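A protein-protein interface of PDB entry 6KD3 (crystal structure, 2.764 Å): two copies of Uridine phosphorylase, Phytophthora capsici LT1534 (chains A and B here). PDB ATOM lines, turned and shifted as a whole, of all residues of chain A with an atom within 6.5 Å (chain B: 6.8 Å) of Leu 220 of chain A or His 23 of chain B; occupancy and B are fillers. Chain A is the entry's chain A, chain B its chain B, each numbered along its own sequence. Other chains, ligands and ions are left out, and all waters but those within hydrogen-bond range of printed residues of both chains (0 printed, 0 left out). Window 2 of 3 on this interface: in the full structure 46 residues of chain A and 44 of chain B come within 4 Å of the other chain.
N of Gly 222 of chain A lies close to ND2 of Asn 21 of chain B, at 2.9 Å.
NH2 of Arg 219 of chain A lies within salt-bridge range of OD2 of Asp 221 of chain A, 3.4 Å away.
The side-chain sulfur of Cys 225 of chain A lies within hydrogen-bond range of the backbone carbonyl oxygen of Tyr 227 of chain A, at 3.5 Å.
OD1 of Asn 21 of chain B is in hydrogen-bond range of N of His 23 of chain B, at 3.0 Å.
N of Ile 24 of chain B is in hydrogen-bond range of OD1 of Asn 21 of chain B, 3.3 Å away.
Among the printed residues, merely in contact across the chains: Cys 225 of chain A with Asn 21 of chain B (3.5 Å), Leu 220 of chain A with His 23 of chain B (3.5 Å), Asp 221 of chain A with Met 27 of chain B (3.6 Å), Asp 221 of chain A with Asn 21 of chain B (3.7 Å), Asp 221 of chain A with Ile 24 of chain B (3.7 Å), Leu 220 of chain A with Asn 21 of chain B (3.7 Å) and Gly 222 of chain A with Ile 24 of chain B (3.9 Å).
Of chain B, only Asn 21 and His 23 come within 4 Å of Leu 220 of chain A.
Of chain A, only Leu 220 comes within 4 Å of His 23 of chain B.
Printed residues of chain B within 4 Å of Gly 222 of chain A: Asn 21 (2.9 Å) and Ile 24 (3.9 Å).
Of the printed residues of chain A, Ile 24 of chain B touches Asp 221 and Gly 222.
The nearest residue of chain B that does not touch Leu 220 of chain A is Ile 24 of chain B (4.6 Å).
The nearest residue of chain A that does not touch His 23 of chain B is Cys 225 of chain A (5.5 Å).
Printed residues of chain A that touch a printed residue of chain B: Leu 220, Asp 221, Gly 222 and Cys 225.
Hydrophobic or aromatic side chains of chain A that line the printed part of chain B: Leu 220.
Along chain A the printed residues that touch a printed residue of chain B span positions 220 to 225.
Of the 7 printed residues of chain B, 4 touch a printed residue of chain A.
Printed residues of chain B that touch a printed residue of chain A: Asn 21, His 23, Ile 24 and Met 27.
Hydrophobic or aromatic side chains of chain B within 4 Å of the printed part of chain A: His 23, Ile 24 and Met 27.
Among the printed residues, no Asp or Glu carboxylate lies within 4 Å of a Lys or Arg side-chain nitrogen of the other chain.
No position is printed for both chains.
Of the 8 pairs that touch across the chains among the printed residues, none has its exchanged pair printed and touching as well.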
ATOM      1  N   TYR A 214      32.588 -26.079 -20.492  1.00  0.00           N
ATOM      2  CA  TYR A 214      31.253 -26.633 -20.313  1.00  0.00           C
ATOM      3  C   TYR A 214      30.583 -26.131 -19.042  1.00  0.00           C
ATOM      4  O   TYR A 214      29.541 -25.465 -19.107  1.00  0.00           O
ATOM      5  CB  TYR A 214      31.301 -28.166 -20.383  1.00  0.00           C
ATOM      6  CG  TYR A 214      31.123 -28.568 -21.819  1.00  0.00           C
ATOM      7  CD1 TYR A 214      29.871 -28.431 -22.453  1.00  0.00           C
ATOM      8  CD2 TYR A 214      32.199 -28.982 -22.575  1.00  0.00           C
ATOM      9  CE1 TYR A 214      29.704 -28.749 -23.793  1.00  0.00           C
ATOM     10  CE2 TYR A 214      32.041 -29.301 -23.918  1.00  0.00           C
ATOM     11  CZ  TYR A 214      30.795 -29.177 -24.513  1.00  0.00           C
ATOM     12  OH  TYR A 214      30.653 -29.494 -25.828  1.00  0.00           O
ATOM     13  N   GLY A 218      28.286 -21.757 -17.935  1.00  0.00           N
ATOM     14  CA  GLY A 218      26.865 -22.046 -17.862  1.00  0.00           C
ATOM     15  C   GLY A 218      26.423 -23.397 -18.416  1.00  0.00           C
ATOM     16  O   GLY A 218      25.511 -24.011 -17.862  1.00  0.00           O
ATOM     17  N   ARG A 219      27.088 -23.911 -19.440  1.00  0.00           N
ATOM     18  CA  ARG A 219      26.410 -24.751 -20.419  1.00  0.00           C
ATOM     19  C   ARG A 219      25.800 -26.029 -19.834  1.00  0.00           C
ATOM     20  O   ARG A 219      26.132 -26.482 -18.736  1.00  0.00           O
ATOM     21  CB  ARG A 219      27.377 -25.094 -21.531  1.00  0.00           C
ATOM     22  CG  ARG A 219      28.120 -23.871 -21.975  1.00  0.00           C
ATOM     23  CD  ARG A 219      29.197 -24.302 -22.844  1.00  0.00           C
ATOM     24  NE  ARG A 219      28.704 -25.189 -23.882  1.00  0.00           N
ATOM     25  CZ  ARG A 219      28.228 -24.780 -25.049  1.00  0.00           C
ATOM     26  NH1 ARG A 219      28.178 -23.488 -25.338  1.00  0.00           N
ATOM     27  NH2 ARG A 219      27.812 -25.675 -25.930  1.00  0.00           N
ATOM     28  N   LEU A 220      24.880 -26.605 -20.612  1.00  0.00           N
ATOM     29  CA  LEU A 220      23.957 -27.652 -20.177  1.00  0.00           C
ATOM     30  C   LEU A 220      24.162 -28.944 -20.952  1.00  0.00           C
ATOM     31  O   LEU A 220      23.229 -29.741 -21.078  1.00  0.00           O
ATOM     32  CB  LEU A 220      22.495 -27.203 -20.332  1.00  0.00           C
ATOM     33  CG  LEU A 220      21.790 -26.290 -19.322  1.00  0.00           C
ATOM     34  CD1 LEU A 220      20.462 -25.660 -19.863  1.00  0.00           C
ATOM     35  CD2 LEU A 220      21.535 -27.093 -18.038  1.00  0.00           C
ATOM     36  N   ASP A 221      25.353 -29.159 -21.492  1.00  0.00           N
ATOM     37  CA  ASP A 221      25.626 -30.343 -22.286  1.00  0.00           C
ATOM     38  C   ASP A 221      27.086 -30.775 -22.093  1.00  0.00           C
ATOM     39  O   ASP A 221      27.833 -31.013 -23.046  1.00  0.00           O
ATOM     40  CB  ASP A 221      25.296 -30.049 -23.741  1.00  0.00           C
ATOM     41  CG  ASP A 221      25.966 -28.809 -24.203  1.00  0.00           C
ATOM     42  OD1 ASP A 221      26.427 -28.094 -23.295  1.00  0.00           O
ATOM     43  OD2 ASP A 221      26.050 -28.541 -25.432  1.00  0.00           O
ATOM     44  N   GLY A 222      27.508 -30.867 -20.838  1.00  0.00           N
ATOM     45  CA  GLY A 222      28.797 -31.417 -20.478  1.00  0.00           C
ATOM     46  C   GLY A 222      28.676 -32.849 -20.004  1.00  0.00           C
ATOM     47  O   GLY A 222      27.935 -33.660 -20.566  1.00  0.00           O
ATOM     48  N   CYS A 225      27.086 -32.012 -14.399  1.00  0.00           N
ATOM     49  CA  CYS A 225      26.116 -30.909 -14.442  1.00  0.00           C
ATOM     50  C   CYS A 225      25.331 -30.834 -13.124  1.00  0.00           C
ATOM     51  O   CYS A 225      24.468 -31.675 -12.854  1.00  0.00           O
ATOM     52  CB  CYS A 225      25.185 -31.098 -15.643  1.00  0.00           C
ATOM     53  SG  CYS A 225      24.378 -29.588 -16.233  1.00  0.00           S
ATOM     54  N   TYR A 227      23.520 -28.046 -11.953  1.00  0.00           N
ATOM     55  CA  TYR A 227      22.675 -26.867 -12.061  1.00  0.00           C
ATOM     56  C   TYR A 227      21.834 -27.066 -13.318  1.00  0.00           C
ATOM     57  O   TYR A 227      22.084 -27.985 -14.103  1.00  0.00           O
ATOM     58  CB  TYR A 227      23.515 -25.592 -12.142  1.00  0.00           C
ATOM     59  CG  TYR A 227      24.532 -25.665 -13.258  1.00  0.00           C
ATOM     60  CD1 TYR A 227      24.128 -25.561 -14.592  1.00  0.00           C
ATOM     61  CD2 TYR A 227      25.892 -25.856 -12.993  1.00  0.00           C
ATOM     62  CE1 TYR A 227      25.035 -25.641 -15.622  1.00  0.00           C
ATOM     63  CE2 TYR A 227      26.814 -25.914 -14.032  1.00  0.00           C
ATOM     64  CZ  TYR A 227      26.369 -25.810 -15.345  1.00  0.00           C
ATOM     65  OH  TYR A 227      27.232 -25.870 -16.407  1.00  0.00           O
ATOM     66  N   THR A 228      20.869 -26.171 -13.541  1.00  0.00           N
ATOM     67  CA  THR A 228      19.943 -26.371 -14.654  1.00  0.00           C
ATOM     68  C   THR A 228      20.067 -25.266 -15.698  1.00  0.00           C
ATOM     69  O   THR A 228      21.175 -24.841 -16.024  1.00  0.00           O
ATOM     70  CB  THR A 228      18.530 -26.453 -14.108  1.00  0.00           C
ATOM     71  OG1 THR A 228      18.363 -25.426 -13.122  1.00  0.00           O
ATOM     72  CG2 THR A 228      18.295 -27.798 -13.480  1.00  0.00           C
ATOM     73  N   LEU A 229      18.931 -24.816 -16.242  1.00  0.00           N
ATOM     74  CA  LEU A 229      18.847 -23.614 -17.066  1.00  0.00           C
ATOM     75  C   LEU A 229      18.415 -22.406 -16.260  1.00  0.00           C
ATOM     76  O   LEU A 229      19.030 -21.339 -16.357  1.00  0.00           O
ATOM     77  CB  LEU A 229      17.870 -23.820 -18.204  1.00  0.00           C
ATOM     78  CG  LEU A 229      17.246 -22.526 -18.690  1.00  0.00           C
ATOM     79  N   GLU A 230      17.380 -22.576 -15.436  1.00  0.00           N
ATOM     80  CA  GLU A 230      16.930 -21.518 -14.526  1.00  0.00           C
ATOM     81  C   GLU A 230      18.072 -20.920 -13.720  1.00  0.00           C
ATOM     82  O   GLU A 230      17.965 -19.783 -13.256  1.00  0.00           O
ATOM     83  CB  GLU A 230      15.855 -22.064 -13.572  1.00  0.00           C
ATOM     84  CG  GLU A 230      16.128 -21.850 -12.071  1.00  0.00           C
ATOM     85  N   LYS A 232      21.586 -21.334 -14.843  1.00  0.00           N
ATOM     86  CA  LYS A 232      22.524 -20.782 -15.822  1.00  0.00           C
ATOM     87  C   LYS A 232      22.035 -19.436 -16.345  1.00  0.00           C
ATOM     88  O   LYS A 232      22.849 -18.557 -16.653  1.00  0.00           O
ATOM     89  CB  LYS A 232      22.715 -21.750 -16.986  1.00  0.00           C
ATOM     90  CG  LYS A 232      23.057 -21.070 -18.330  1.00  0.00           C
ATOM     91  CD  LYS A 232      22.969 -22.045 -19.491  1.00  0.00           C
ATOM     92  CE  LYS A 232      22.142 -21.523 -20.626  1.00  0.00           C
ATOM     93  NZ  LYS A 232      21.758 -22.638 -21.532  1.00  0.00           N
ATOM     94  N   ARG A 275      24.002 -16.360 -25.809  1.00  0.00           N
ATOM     95  CA  ARG A 275      23.603 -17.488 -24.964  1.00  0.00           C
ATOM     96  C   ARG A 275      22.442 -17.173 -24.063  1.00  0.00           C
ATOM     97  O   ARG A 275      22.095 -18.029 -23.233  1.00  0.00           O
ATOM     98  CB  ARG A 275      24.772 -17.933 -24.102  1.00  0.00           C
ATOM     99  CG  ARG A 275      25.993 -18.240 -24.915  1.00  0.00           C
ATOM    100  CD  ARG A 275      27.206 -18.440 -24.015  1.00  0.00           C
ATOM    101  NE  ARG A 275      26.883 -18.919 -22.660  1.00  0.00           N
ATOM    102  CZ  ARG A 275      26.576 -20.172 -22.349  1.00  0.00           C
ATOM    103  NH1 ARG A 275      26.494 -21.105 -23.283  1.00  0.00           N
ATOM    104  NH2 ARG A 275      26.338 -20.475 -21.094  1.00  0.00           N
ATOM    105  N   ASP A 279      22.533 -22.567 -26.143  1.00  0.00           N
ATOM    106  CA  ASP A 279      23.838 -23.138 -25.808  1.00  0.00           C
ATOM    107  C   ASP A 279      24.492 -23.779 -27.028  1.00  0.00           C
ATOM    108  O   ASP A 279      25.695 -24.083 -27.014  1.00  0.00           O
ATOM    109  CB  ASP A 279      23.708 -24.171 -24.695  1.00  0.00           C
ATOM    110  CG  ASP A 279      23.793 -23.555 -23.348  1.00  0.00           C
ATOM    111  OD1 ASP A 279      24.473 -22.515 -23.262  1.00  0.00           O
ATOM    112  OD2 ASP A 279      23.192 -24.076 -22.379  1.00  0.00           O
ATOM    113  N   ASN B  21      25.212 -35.765 -16.224  1.00  0.00           N
ATOM    114  CA  ASN B  21      24.468 -34.699 -16.894  1.00  0.00           C
ATOM    115  C   ASN B  21      23.073 -35.215 -17.194  1.00  0.00           C
ATOM    116  O   ASN B  21      22.923 -36.209 -17.909  1.00  0.00           O
ATOM    117  CB  ASN B  21      25.178 -34.268 -18.184  1.00  0.00           C
ATOM    118  CG  ASN B  21      24.678 -32.941 -18.716  1.00  0.00           C
ATOM    119  OD1 ASN B  21      23.480 -32.752 -18.899  1.00  0.00           O
ATOM    120  ND2 ASN B  21      25.593 -32.017 -18.985  1.00  0.00           N
ATOM    121  N   SER B  22      22.057 -34.551 -16.660  1.00  0.00           N
ATOM    122  CA  SER B  22      20.698 -35.010 -16.895  1.00  0.00           C
ATOM    123  C   SER B  22      20.169 -34.530 -18.244  1.00  0.00           C
ATOM    124  O   SER B  22      19.478 -35.276 -18.947  1.00  0.00           O
ATOM    125  CB  SER B  22      19.809 -34.532 -15.752  1.00  0.00           C
ATOM    126  OG  SER B  22      20.402 -34.846 -14.500  1.00  0.00           O
ATOM    127  N   HIS B  23      20.493 -33.296 -18.625  1.00  0.00           N
ATOM    128  CA  HIS B  23      19.952 -32.689 -19.837  1.00  0.00           C
ATOM    129  C   HIS B  23      20.493 -33.319 -21.111  1.00  0.00           C
ATOM    130  O   HIS B  23      20.089 -32.912 -22.203  1.00  0.00           O
ATOM    131  CB  HIS B  23      20.252 -31.187 -19.852  1.00  0.00           C
ATOM    132  CG  HIS B  23      19.568 -30.422 -18.760  1.00  0.00           C
ATOM    133  N   ILE B  24      21.390 -34.296 -21.001  1.00  0.00           N
ATOM    134  CA  ILE B  24      21.925 -34.953 -22.189  1.00  0.00           C
ATOM    135  C   ILE B  24      20.899 -35.916 -22.786  1.00  0.00           C
ATOM    136  O   ILE B  24      20.920 -36.200 -23.992  1.00  0.00           O
ATOM    137  CB  ILE B  24      23.261 -35.630 -21.816  1.00  0.00           C
ATOM    138  CG1 ILE B  24      24.375 -34.579 -21.813  1.00  0.00           C
ATOM    139  CG2 ILE B  24      23.574 -36.823 -22.723  1.00  0.00           C
ATOM    140  CD1 ILE B  24      24.383 -33.731 -23.068  1.00  0.00           C
ATOM    141  N   LEU B  25      19.968 -36.401 -21.965  1.00  0.00           N
ATOM    142  CA  LEU B  25      18.889 -37.247 -22.465  1.00  0.00           C
ATOM    143  C   LEU B  25      17.841 -36.431 -23.210  1.00  0.00           C
ATOM    144  O   LEU B  25      17.399 -36.825 -24.295  1.00  0.00           O
ATOM    145  CB  LEU B  25      18.245 -38.012 -21.304  1.00  0.00           C
ATOM    146  N   GLU B  26      17.431 -35.299 -22.639  1.00  0.00           N
ATOM    147  CA  GLU B  26      16.489 -34.391 -23.292  1.00  0.00           C
ATOM    148  C   GLU B  26      17.258 -33.486 -24.259  1.00  0.00           C
ATOM    149  O   GLU B  26      17.466 -32.292 -24.030  1.00  0.00           O
ATOM    150  CB  GLU B  26      15.722 -33.596 -22.246  1.00  0.00           C
ATOM    151  CG  GLU B  26      14.921 -34.473 -21.306  1.00  0.00           C
ATOM    152  N   MET B  27      17.685 -34.100 -25.363  1.00  0.00           N
ATOM    153  CA  MET B  27      18.501 -33.445 -26.376  1.00  0.00           C
ATOM    154  C   MET B  27      18.329 -34.193 -27.692  1.00  0.00           C
ATOM    155  O   MET B  27      18.383 -35.423 -27.712  1.00  0.00           O
ATOM    156  CB  MET B  27      19.984 -33.424 -25.970  1.00  0.00           C
ATOM    157  CG  MET B  27      20.429 -32.156 -25.244  1.00  0.00           C
ATOM    158  SD  MET B  27      22.227 -31.971 -25.129  1.00  0.00           S
ATOM    159  CE  MET B  27      22.392 -30.325 -25.824  1.00  0.00           C
